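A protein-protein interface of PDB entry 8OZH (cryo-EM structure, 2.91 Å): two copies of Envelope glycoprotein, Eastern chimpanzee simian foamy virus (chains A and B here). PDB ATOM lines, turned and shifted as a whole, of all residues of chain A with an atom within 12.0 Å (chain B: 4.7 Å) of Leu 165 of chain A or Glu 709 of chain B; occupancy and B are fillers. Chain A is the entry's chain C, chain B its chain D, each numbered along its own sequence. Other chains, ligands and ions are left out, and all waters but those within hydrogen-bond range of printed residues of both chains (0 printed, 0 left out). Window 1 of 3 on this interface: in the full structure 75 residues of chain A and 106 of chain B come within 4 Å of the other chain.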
ATOM      1  N   VAL A 159     -11.832   0.700 -13.761  1.00  0.00           N
ATOM      2  CA  VAL A 159     -12.124   2.140 -13.482  1.00  0.00           C
ATOM      3  C   VAL A 159     -13.612   2.399 -13.741  1.00  0.00           C
ATOM      4  O   VAL A 159     -14.084   2.060 -14.838  1.00  0.00           O
ATOM      5  CB  VAL A 159     -11.250   3.056 -14.358  1.00  0.00           C
ATOM      6  CG1 VAL A 159     -11.638   4.516 -14.205  1.00  0.00           C
ATOM      7  CG2 VAL A 159      -9.772   2.870 -14.077  1.00  0.00           C
ATOM      8  N   VAL A 160     -14.315   2.993 -12.772  1.00  0.00           N
ATOM      9  CA  VAL A 160     -15.724   3.468 -12.932  1.00  0.00           C
ATOM     10  C   VAL A 160     -15.663   4.932 -13.370  1.00  0.00           C
ATOM     11  O   VAL A 160     -15.002   5.727 -12.675  1.00  0.00           O
ATOM     12  CB  VAL A 160     -16.573   3.313 -11.655  1.00  0.00           C
ATOM     13  CG1 VAL A 160     -18.047   3.470 -11.969  1.00  0.00           C
ATOM     14  CG2 VAL A 160     -16.331   1.984 -10.958  1.00  0.00           C
ATOM     15  N   LYS A 161     -16.322   5.251 -14.482  1.00  0.00           N
ATOM     16  CA  LYS A 161     -16.346   6.603 -15.094  1.00  0.00           C
ATOM     17  C   LYS A 161     -17.320   7.486 -14.322  1.00  0.00           C
ATOM     18  O   LYS A 161     -18.476   7.058 -14.154  1.00  0.00           O
ATOM     19  CB  LYS A 161     -16.802   6.495 -16.548  1.00  0.00           C
ATOM     20  CG  LYS A 161     -16.830   7.799 -17.327  1.00  0.00           C
ATOM     21  CD  LYS A 161     -17.409   7.636 -18.712  1.00  0.00           C
ATOM     22  CE  LYS A 161     -16.574   6.743 -19.603  1.00  0.00           C
ATOM     23  NZ  LYS A 161     -17.087   6.758 -20.991  1.00  0.00           N
ATOM     24  N   GLU A 162     -16.880   8.672 -13.908  1.00  0.00           N
ATOM     25  CA  GLU A 162     -17.764   9.745 -13.379  1.00  0.00           C
ATOM     26  C   GLU A 162     -18.276  10.621 -14.535  1.00  0.00           C
ATOM     27  O   GLU A 162     -19.497  10.831 -14.628  1.00  0.00           O
ATOM     28  CB  GLU A 162     -17.008  10.599 -12.367  1.00  0.00           C
ATOM     29  CG  GLU A 162     -17.931  11.376 -11.467  1.00  0.00           C
ATOM     30  CD  GLU A 162     -17.326  11.685 -10.109  1.00  0.00           C
ATOM     31  OE1 GLU A 162     -16.182  12.214 -10.076  1.00  0.00           O
ATOM     32  OE2 GLU A 162     -17.994  11.388  -9.083  1.00  0.00           O
ATOM     33  N   ARG A 163     -17.356  11.071 -15.390  1.00  0.00           N
ATOM     34  CA  ARG A 163     -17.505  12.182 -16.363  1.00  0.00           C
ATOM     35  C   ARG A 163     -16.348  12.119 -17.353  1.00  0.00           C
ATOM     36  O   ARG A 163     -15.431  11.314 -17.122  1.00  0.00           O
ATOM     37  CB  ARG A 163     -17.354  13.530 -15.656  1.00  0.00           C
ATOM     38  CG  ARG A 163     -18.663  14.177 -15.274  1.00  0.00           C
ATOM     39  CD  ARG A 163     -18.421  15.505 -14.595  1.00  0.00           C
ATOM     40  NE  ARG A 163     -18.269  15.355 -13.158  1.00  0.00           N
ATOM     41  CZ  ARG A 163     -19.237  15.022 -12.306  1.00  0.00           C
ATOM     42  NH1 ARG A 163     -20.461  14.759 -12.728  1.00  0.00           N
ATOM     43  NH2 ARG A 163     -18.965  14.932 -11.016  1.00  0.00           N
ATOM     44  N   VAL A 164     -16.362  12.998 -18.355  1.00  0.00           N
ATOM     45  CA  VAL A 164     -15.234  13.220 -19.306  1.00  0.00           C
ATOM     46  C   VAL A 164     -15.007  14.726 -19.425  1.00  0.00           C
ATOM     47  O   VAL A 164     -15.996  15.466 -19.567  1.00  0.00           O
ATOM     48  CB  VAL A 164     -15.525  12.579 -20.672  1.00  0.00           C
ATOM     49  CG1 VAL A 164     -14.410  12.845 -21.660  1.00  0.00           C
ATOM     50  CG2 VAL A 164     -15.759  11.090 -20.539  1.00  0.00           C
ATOM     51  N   LEU A 165     -13.749  15.150 -19.357  1.00  0.00           N
ATOM     52  CA  LEU A 165     -13.312  16.541 -19.640  1.00  0.00           C
ATOM     53  C   LEU A 165     -12.745  16.555 -21.053  1.00  0.00           C
ATOM     54  O   LEU A 165     -12.017  15.620 -21.372  1.00  0.00           O
ATOM     55  CB  LEU A 165     -12.251  16.931 -18.609  1.00  0.00           C
ATOM     56  CG  LEU A 165     -11.607  18.301 -18.792  1.00  0.00           C
ATOM     57  CD1 LEU A 165     -12.652  19.406 -18.799  1.00  0.00           C
ATOM     58  CD2 LEU A 165     -10.577  18.533 -17.697  1.00  0.00           C
ATOM     59  N   GLY A 166     -13.097  17.552 -21.864  1.00  0.00           N
ATOM     60  CA  GLY A 166     -12.570  17.758 -23.229  1.00  0.00           C
ATOM     61  C   GLY A 166     -11.754  19.038 -23.312  1.00  0.00           C
ATOM     62  O   GLY A 166     -12.228  20.070 -22.810  1.00  0.00           O
ATOM     63  N   LEU A 167     -10.578  18.982 -23.932  1.00  0.00           N
ATOM     64  CA  LEU A 167      -9.609  20.104 -24.062  1.00  0.00           C
ATOM     65  C   LEU A 167      -9.216  20.269 -25.532  1.00  0.00           C
ATOM     66  O   LEU A 167      -9.223  19.261 -26.258  1.00  0.00           O
ATOM     67  CB  LEU A 167      -8.362  19.764 -23.249  1.00  0.00           C
ATOM     68  CG  LEU A 167      -8.349  20.281 -21.824  1.00  0.00           C
ATOM     69  CD1 LEU A 167      -7.255  19.600 -21.019  1.00  0.00           C
ATOM     70  CD2 LEU A 167      -8.129  21.779 -21.825  1.00  0.00           C
ATOM     71  N   SER A 168      -8.837  21.482 -25.926  1.00  0.00           N
ATOM     72  CA  SER A 168      -8.217  21.796 -27.235  1.00  0.00           C
ATOM     73  C   SER A 168      -6.903  22.535 -26.993  1.00  0.00           C
ATOM     74  O   SER A 168      -6.953  23.605 -26.391  1.00  0.00           O
ATOM     75  CB  SER A 168      -9.146  22.603 -28.075  1.00  0.00           C
ATOM     76  OG  SER A 168      -8.556  22.906 -29.330  1.00  0.00           O
ATOM     77  N   GLN A 169      -5.780  21.972 -27.438  1.00  0.00           N
ATOM     78  CA  GLN A 169      -4.443  22.613 -27.373  1.00  0.00           C
ATOM     79  C   GLN A 169      -3.960  22.906 -28.792  1.00  0.00           C
ATOM     80  O   GLN A 169      -4.083  22.004 -29.631  1.00  0.00           O
ATOM     81  CB  GLN A 169      -3.450  21.711 -26.656  1.00  0.00           C
ATOM     82  CG  GLN A 169      -2.128  22.407 -26.397  1.00  0.00           C
ATOM     83  CD  GLN A 169      -1.147  21.571 -25.613  1.00  0.00           C
ATOM     84  OE1 GLN A 169      -1.110  20.343 -25.713  1.00  0.00           O
ATOM     85  NE2 GLN A 169      -0.328  22.250 -24.826  1.00  0.00           N
ATOM     86  N   PHE A 210     -11.225  17.020 -38.674  1.00  0.00           N
ATOM     87  CA  PHE A 210     -12.409  16.822 -37.803  1.00  0.00           C
ATOM     88  C   PHE A 210     -12.902  18.186 -37.308  1.00  0.00           C
ATOM     89  O   PHE A 210     -12.072  18.985 -36.869  1.00  0.00           O
ATOM     90  CB  PHE A 210     -12.021  15.930 -36.626  1.00  0.00           C
ATOM     91  CG  PHE A 210     -12.020  14.455 -36.932  1.00  0.00           C
ATOM     92  CD1 PHE A 210     -10.940  13.860 -37.569  1.00  0.00           C
ATOM     93  CD2 PHE A 210     -13.095  13.652 -36.567  1.00  0.00           C
ATOM     94  CE1 PHE A 210     -10.946  12.502 -37.852  1.00  0.00           C
ATOM     95  CE2 PHE A 210     -13.097  12.295 -36.849  1.00  0.00           C
ATOM     96  CZ  PHE A 210     -12.020  11.721 -37.492  1.00  0.00           C
ATOM     97  N   GLU A 211     -14.206  18.448 -37.373  1.00  0.00           N
ATOM     98  CA  GLU A 211     -14.859  19.636 -36.755  1.00  0.00           C
ATOM     99  C   GLU A 211     -14.920  19.434 -35.232  1.00  0.00           C
ATOM    100  O   GLU A 211     -15.379  18.359 -34.808  1.00  0.00           O
ATOM    101  CB  GLU A 211     -16.257  19.811 -37.358  1.00  0.00           C
ATOM    102  CG  GLU A 211     -17.184  20.713 -36.572  1.00  0.00           C
ATOM    103  CD  GLU A 211     -17.110  22.170 -36.981  1.00  0.00           C
ATOM    104  OE1 GLU A 211     -15.988  22.723 -36.985  1.00  0.00           O
ATOM    105  OE2 GLU A 211     -18.174  22.746 -37.305  1.00  0.00           O
ATOM    106  N   ILE A 212     -14.510  20.432 -34.449  1.00  0.00           N
ATOM    107  CA  ILE A 212     -14.574  20.444 -32.955  1.00  0.00           C
ATOM    108  C   ILE A 212     -15.489  21.598 -32.539  1.00  0.00           C
ATOM    109  O   ILE A 212     -15.266  22.734 -32.950  1.00  0.00           O
ATOM    110  CB  ILE A 212     -13.154  20.584 -32.369  1.00  0.00           C
ATOM    111  CG1 ILE A 212     -12.228  19.456 -32.834  1.00  0.00           C
ATOM    112  CG2 ILE A 212     -13.175  20.700 -30.855  1.00  0.00           C
ATOM    113  CD1 ILE A 212     -12.678  18.062 -32.449  1.00  0.00           C
ATOM    114  N   PRO A 213     -16.533  21.381 -31.707  1.00  0.00           N
ATOM    115  CA  PRO A 213     -17.565  22.399 -31.498  1.00  0.00           C
ATOM    116  C   PRO A 213     -17.236  23.470 -30.442  1.00  0.00           C
ATOM    117  O   PRO A 213     -18.013  23.635 -29.522  1.00  0.00           O
ATOM    118  CB  PRO A 213     -18.739  21.506 -31.069  1.00  0.00           C
ATOM    119  CG  PRO A 213     -18.081  20.466 -30.200  1.00  0.00           C
ATOM    120  CD  PRO A 213     -16.787  20.159 -30.925  1.00  0.00           C
ATOM    121  N   LEU A 214     -16.109  24.175 -30.599  1.00  0.00           N
ATOM    122  CA  LEU A 214     -15.750  25.401 -29.833  1.00  0.00           C
ATOM    123  C   LEU A 214     -15.639  26.577 -30.807  1.00  0.00           C
ATOM    124  O   LEU A 214     -15.711  26.339 -32.026  1.00  0.00           O
ATOM    125  CB  LEU A 214     -14.413  25.188 -29.125  1.00  0.00           C
ATOM    126  CG  LEU A 214     -14.362  24.073 -28.089  1.00  0.00           C
ATOM    127  CD1 LEU A 214     -12.926  23.812 -27.663  1.00  0.00           C
ATOM    128  CD2 LEU A 214     -15.225  24.414 -26.886  1.00  0.00           C
ATOM    129  N   TYR B 585     -17.404  14.238 -33.849  1.00  0.00           N
ATOM    130  CA  TYR B 585     -17.345  14.806 -32.472  1.00  0.00           C
ATOM    131  C   TYR B 585     -18.258  16.034 -32.354  1.00  0.00           C
ATOM    132  O   TYR B 585     -18.134  16.758 -31.349  1.00  0.00           O
ATOM    133  CB  TYR B 585     -15.896  15.101 -32.081  1.00  0.00           C
ATOM    134  CG  TYR B 585     -15.058  13.859 -31.945  1.00  0.00           C
ATOM    135  CD1 TYR B 585     -14.389  13.323 -33.035  1.00  0.00           C
ATOM    136  CD2 TYR B 585     -14.974  13.184 -30.740  1.00  0.00           C
ATOM    137  CE1 TYR B 585     -13.641  12.162 -32.927  1.00  0.00           C
ATOM    138  CE2 TYR B 585     -14.221  12.026 -30.608  1.00  0.00           C
ATOM    139  CZ  TYR B 585     -13.551  11.512 -31.707  1.00  0.00           C
ATOM    140  OH  TYR B 585     -12.812  10.371 -31.585  1.00  0.00           O
ATOM    141  N   ILE B 597     -11.117  24.481 -15.634  1.00  0.00           N
ATOM    142  CA  ILE B 597     -10.959  23.003 -15.458  1.00  0.00           C
ATOM    143  C   ILE B 597     -11.522  22.601 -14.085  1.00  0.00           C
ATOM    144  O   ILE B 597     -12.207  21.564 -14.019  1.00  0.00           O
ATOM    145  CB  ILE B 597      -9.496  22.559 -15.652  1.00  0.00           C
ATOM    146  CG1 ILE B 597      -9.070  22.701 -17.112  1.00  0.00           C
ATOM    147  CG2 ILE B 597      -9.285  21.138 -15.153  1.00  0.00           C
ATOM    148  CD1 ILE B 597      -7.620  22.362 -17.365  1.00  0.00           C
ATOM    149  N   ILE B 600     -15.077  20.993 -13.244  1.00  0.00           N
ATOM    150  CA  ILE B 600     -15.416  19.573 -13.556  1.00  0.00           C
ATOM    151  C   ILE B 600     -15.806  18.816 -12.271  1.00  0.00           C
ATOM    152  O   ILE B 600     -16.557  17.820 -12.384  1.00  0.00           O
ATOM    153  CB  ILE B 600     -14.257  18.897 -14.314  1.00  0.00           C
ATOM    154  CG1 ILE B 600     -14.689  17.612 -15.025  1.00  0.00           C
ATOM    155  CG2 ILE B 600     -13.081  18.637 -13.386  1.00  0.00           C
ATOM    156  CD1 ILE B 600     -15.634  17.810 -16.181  1.00  0.00           C
ATOM    157  N   ILE B 609     -20.023  14.633 -21.401  1.00  0.00           N
ATOM    158  CA  ILE B 609     -18.812  15.313 -21.942  1.00  0.00           C
ATOM    159  C   ILE B 609     -18.972  16.814 -21.691  1.00  0.00           C
ATOM    160  O   ILE B 609     -19.949  17.387 -22.192  1.00  0.00           O
ATOM    161  CB  ILE B 609     -18.610  14.998 -23.441  1.00  0.00           C
ATOM    162  CG1 ILE B 609     -18.581  13.492 -23.706  1.00  0.00           C
ATOM    163  CG2 ILE B 609     -17.348  15.661 -23.961  1.00  0.00           C
ATOM    164  CD1 ILE B 609     -19.922  12.874 -24.008  1.00  0.00           C
ATOM    165  N   TYR B 610     -18.029  17.424 -20.983  1.00  0.00           N
ATOM    166  CA  TYR B 610     -17.975  18.883 -20.747  1.00  0.00           C
ATOM    167  C   TYR B 610     -16.668  19.424 -21.321  1.00  0.00           C
ATOM    168  O   TYR B 610     -15.608  18.947 -20.900  1.00  0.00           O
ATOM    169  CB  TYR B 610     -18.091  19.180 -19.254  1.00  0.00           C
ATOM    170  CG  TYR B 610     -19.332  18.624 -18.605  1.00  0.00           C
ATOM    171  CD1 TYR B 610     -20.527  19.324 -18.611  1.00  0.00           C
ATOM    172  CD2 TYR B 610     -19.311  17.389 -17.982  1.00  0.00           C
ATOM    173  CE1 TYR B 610     -21.661  18.816 -17.999  1.00  0.00           C
ATOM    174  CE2 TYR B 610     -20.440  16.861 -17.372  1.00  0.00           C
ATOM    175  CZ  TYR B 610     -21.617  17.583 -17.371  1.00  0.00           C
ATOM    176  OH  TYR B 610     -22.716  17.054 -16.758  1.00  0.00           O
ATOM    177  N   LEU B 612     -13.867  22.475 -21.981  1.00  0.00           N
ATOM    178  CA  LEU B 612     -13.288  23.755 -21.497  1.00  0.00           C
ATOM    179  C   LEU B 612     -13.474  24.793 -22.609  1.00  0.00           C
ATOM    180  O   LEU B 612     -13.161  24.468 -23.759  1.00  0.00           O
ATOM    181  CB  LEU B 612     -11.812  23.527 -21.163  1.00  0.00           C
ATOM    182  CG  LEU B 612     -11.071  24.734 -20.609  1.00  0.00           C
ATOM    183  CD1 LEU B 612     -11.580  25.076 -19.227  1.00  0.00           C
ATOM    184  CD2 LEU B 612      -9.582  24.471 -20.579  1.00  0.00           C
ATOM    185  N   LEU B 669      -7.258  19.900 -11.279  1.00  0.00           N
ATOM    186  CA  LEU B 669      -8.089  18.677 -11.082  1.00  0.00           C
ATOM    187  C   LEU B 669      -8.302  18.375  -9.591  1.00  0.00           C
ATOM    188  O   LEU B 669      -9.303  17.698  -9.299  1.00  0.00           O
ATOM    189  CB  LEU B 669      -7.452  17.478 -11.789  1.00  0.00           C
ATOM    190  CG  LEU B 669      -7.516  17.495 -13.314  1.00  0.00           C
ATOM    191  CD1 LEU B 669      -6.852  16.254 -13.878  1.00  0.00           C
ATOM    192  CD2 LEU B 669      -8.949  17.603 -13.817  1.00  0.00           C
ATOM    193  N   ALA B 683      -6.024   8.522 -20.704  1.00  0.00           N
ATOM    194  CA  ALA B 683      -6.422   9.645 -21.591  1.00  0.00           C
ATOM    195  C   ALA B 683      -6.054   9.320 -23.051  1.00  0.00           C
ATOM    196  O   ALA B 683      -5.068   8.603 -23.251  1.00  0.00           O
ATOM    197  CB  ALA B 683      -5.780  10.926 -21.110  1.00  0.00           C
ATOM    198  N   ARG B 684      -6.804   9.850 -24.024  1.00  0.00           N
ATOM    199  CA  ARG B 684      -6.640   9.584 -25.485  1.00  0.00           C
ATOM    200  C   ARG B 684      -6.635  10.907 -26.268  1.00  0.00           C
ATOM    201  O   ARG B 684      -7.341  11.833 -25.839  1.00  0.00           O
ATOM    202  CB  ARG B 684      -7.757   8.657 -25.975  1.00  0.00           C
ATOM    203  CG  ARG B 684      -7.640   7.219 -25.486  1.00  0.00           C
ATOM    204  CD  ARG B 684      -6.493   6.441 -26.130  1.00  0.00           C
ATOM    205  NE  ARG B 684      -6.173   5.162 -25.498  1.00  0.00           N
ATOM    206  CZ  ARG B 684      -5.464   5.000 -24.372  1.00  0.00           C
ATOM    207  NH1 ARG B 684      -4.996   6.040 -23.702  1.00  0.00           N
ATOM    208  NH2 ARG B 684      -5.233   3.782 -23.907  1.00  0.00           N
ATOM    209  N   TYR B 707      -6.969  17.574 -29.807  1.00  0.00           N
ATOM    210  CA  TYR B 707      -8.180  17.461 -28.945  1.00  0.00           C
ATOM    211  C   TYR B 707      -8.007  16.272 -27.994  1.00  0.00           C
ATOM    212  O   TYR B 707      -7.752  15.160 -28.514  1.00  0.00           O
ATOM    213  CB  TYR B 707      -9.430  17.324 -29.816  1.00  0.00           C
ATOM    214  CG  TYR B 707     -10.699  16.966 -29.080  1.00  0.00           C
ATOM    215  CD1 TYR B 707     -11.339  17.881 -28.260  1.00  0.00           C
ATOM    216  CD2 TYR B 707     -11.286  15.718 -29.238  1.00  0.00           C
ATOM    217  CE1 TYR B 707     -12.504  17.553 -27.587  1.00  0.00           C
ATOM    218  CE2 TYR B 707     -12.458  15.375 -28.579  1.00  0.00           C
ATOM    219  CZ  TYR B 707     -13.068  16.295 -27.741  1.00  0.00           C
ATOM    220  OH  TYR B 707     -14.226  15.958 -27.091  1.00  0.00           O
ATOM    221  N   TYR B 708      -8.098  16.503 -26.673  1.00  0.00           N
ATOM    222  CA  TYR B 708      -7.894  15.489 -25.598  1.00  0.00           C
ATOM    223  C   TYR B 708      -9.213  15.164 -24.885  1.00  0.00           C
ATOM    224  O   TYR B 708     -10.019  16.079 -24.674  1.00  0.00           O
ATOM    225  CB  TYR B 708      -6.928  15.981 -24.524  1.00  0.00           C
ATOM    226  CG  TYR B 708      -5.579  16.446 -25.005  1.00  0.00           C
ATOM    227  CD1 TYR B 708      -4.888  15.788 -26.012  1.00  0.00           C
ATOM    228  CD2 TYR B 708      -4.954  17.527 -24.399  1.00  0.00           C
ATOM    229  CE1 TYR B 708      -3.635  16.219 -26.426  1.00  0.00           C
ATOM    230  CE2 TYR B 708      -3.700  17.962 -24.795  1.00  0.00           C
ATOM    231  CZ  TYR B 708      -3.037  17.309 -25.815  1.00  0.00           C
ATOM    232  OH  TYR B 708      -1.805  17.750 -26.201  1.00  0.00           O
ATOM    233  N   GLU B 709      -9.420  13.895 -24.527  1.00  0.00           N
ATOM    234  CA  GLU B 709     -10.574  13.445 -23.703  1.00  0.00           C
ATOM    235  C   GLU B 709     -10.040  12.695 -22.485  1.00  0.00           C
ATOM    236  O   GLU B 709      -9.521  11.577 -22.650  1.00  0.00           O
ATOM    237  CB  GLU B 709     -11.535  12.571 -24.504  1.00  0.00           C
ATOM    238  CG  GLU B 709     -12.322  13.341 -25.549  1.00  0.00           C
ATOM    239  CD  GLU B 709     -13.600  12.647 -26.001  1.00  0.00           C
ATOM    240  OE1 GLU B 709     -13.605  11.390 -26.056  1.00  0.00           O
ATOM    241  OE2 GLU B 709     -14.598  13.365 -26.284  1.00  0.00           O
ATOM    242  N   LEU B 710     -10.162  13.327 -21.320  1.00  0.00           N
ATOM    243  CA  LEU B 710      -9.723  12.810 -20.006  1.00  0.00           C
ATOM    244  C   LEU B 710     -10.937  12.205 -19.297  1.00  0.00           C
ATOM    245  O   LEU B 710     -11.876  12.960 -19.010  1.00  0.00           O
ATOM    246  CB  LEU B 710      -9.127  13.965 -19.202  1.00  0.00           C
ATOM    247  CG  LEU B 710      -7.659  14.266 -19.477  1.00  0.00           C
ATOM    248  CD1 LEU B 710      -7.411  14.474 -20.954  1.00  0.00           C
ATOM    249  CD2 LEU B 710      -7.204  15.478 -18.685  1.00  0.00           C
ATOM    250  N   VAL B 711     -10.930  10.892 -19.070  1.00  0.00           N
ATOM    251  CA  VAL B 711     -11.899  10.184 -18.185  1.00  0.00           C
ATOM    252  C   VAL B 711     -11.544  10.547 -16.739  1.00  0.00           C
ATOM    253  O   VAL B 711     -10.399  10.293 -16.351  1.00  0.00           O
ATOM    254  CB  VAL B 711     -11.839   8.662 -18.413  1.00  0.00           C
ATOM    255  CG1 VAL B 711     -12.642   7.883 -17.381  1.00  0.00           C
ATOM    256  CG2 VAL B 711     -12.271   8.290 -19.815  1.00  0.00           C
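The guanidinium group (NE) of Arg 163 of chain A sits at hydrogen-bond distance from the backbone carbonyl oxygen (O) of Ile 600 of chain B (3.1 Å).
The backbone carbonyl oxygen of Val 164 of chain A sits at hydrogen-bond distance from the backbone NH of Tyr 610 of chain B, 3.2 Å away.
The backbone carbonyl oxygen (O) of Leu 710 of chain B sits at hydrogen-bond distance from the backbone NH (N) of Leu 165 of chain A, at 2.9 Å.
The backbone carbonyl oxygen (O) of Tyr 610 of chain B is in hydrogen-bond range of the backbone NH (N) of Gly 166 of chain A, 3.0 Å away.
N of Leu 612 of chain B is in hydrogen-bond range of O of Gly 166 of chain A.
The backbone carbonyl oxygen (O) of Leu 167 of chain A is in hydrogen-bond range of the backbone NH (N) of Tyr 708 of chain B (3.0 Å).
OH of Tyr 708 of chain B sits at hydrogen-bond distance from OE1 of Gln 169 of chain A (2.7 Å).
N of Glu 709 of chain B is in hydrogen-bond range of O of Arg 684 of chain B (3.2 Å).
OH of Tyr 707 of chain B lies within hydrogen-bond range of OE2 of Glu 709 of chain B, at 2.7 Å.
Among the printed residues, pairs that only touch across the chains: Leu 167 of chain A with Tyr 707 of chain B, Leu 167 of chain A with Leu 612 of chain B, Gly 166 of chain A with Tyr 708 of chain B, Val 164 of chain A with Leu 710 of chain B, Leu 165 of chain A with Glu 709 of chain B, Leu 165 of chain A with Tyr 610 of chain B, Pro 213 of chain A with Tyr 585 of chain B, Val 164 of chain A with Ile 609 of chain B, Arg 163 of chain A with Tyr 610 of chain B, Leu 214 of chain A with Leu 612 of chain B, Phe 210 of chain A with Tyr 585 of chain B, Arg 163 of chain A with Val 711 of chain B, Leu 165 of chain A with Ile 597 of chain B and Leu 165 of chain A with Tyr 708 of chain B.
Printed residues of chain B within 4 Å of Val 164 of chain A: Ile 609, Tyr 610 and Leu 710.
Of chain B, only Ile 597 (3.9 Å), Tyr 610 (3.6 Å), Tyr 708 (3.9 Å), Glu 709 (3.5 Å) and Leu 710 (2.9 Å) come within 4 Å of Leu 165 of chain A.
Of the printed residues of chain B, Gly 166 of chain A touches Tyr 610 (3.0 Å), Leu 612 (3.0 Å) and Tyr 708 (3.4 Å).
Of the printed residues of chain B, Phe 210 of chain A touches Tyr 585 (3.8 Å).
Of the printed residues of chain B, Pro 213 of chain A touches Tyr 585.
Ile 609 of chain B touches just one residue of chain A: Val 164 (3.7 Å).
Printed residues of chain A within 4 Å of Tyr 610 of chain B: Arg 163, Val 164, Leu 165 and Gly 166.
Leu 612 of chain B touches just these residues of chain A: Gly 166, Leu 167 and Leu 214.
Leu 669 of chain B touches none of the printed residues of chain A.
No residue of chain A comes within 4 Å of Ala 683 of chain B.
Arg 684 of chain B touches none of the printed residues of chain A.
Tyr 707 of chain B touches one residue of chain A.
Of chain A, only Val 164 and Leu 165 come within 4 Å of Leu 710 of chain B.
Of chain A, only Arg 163 (3.9 Å) comes within 4 Å of Val 711 of chain B.
The nearest printed residue of chain B that does not touch Pro 213 of chain A is Tyr 707 of chain B (6.0 Å).
Among the printed residues, 21 pairs touch across the chains.
Among the printed residues, no Asp or Glu carboxylate lies within 4 Å of a Lys or Arg side-chain nitrogen of the other chain.
No position is printed for both chains.
Of the 21 pairs that touch across the chains among the printed residues, none has its exchanged pair printed and touching as well.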
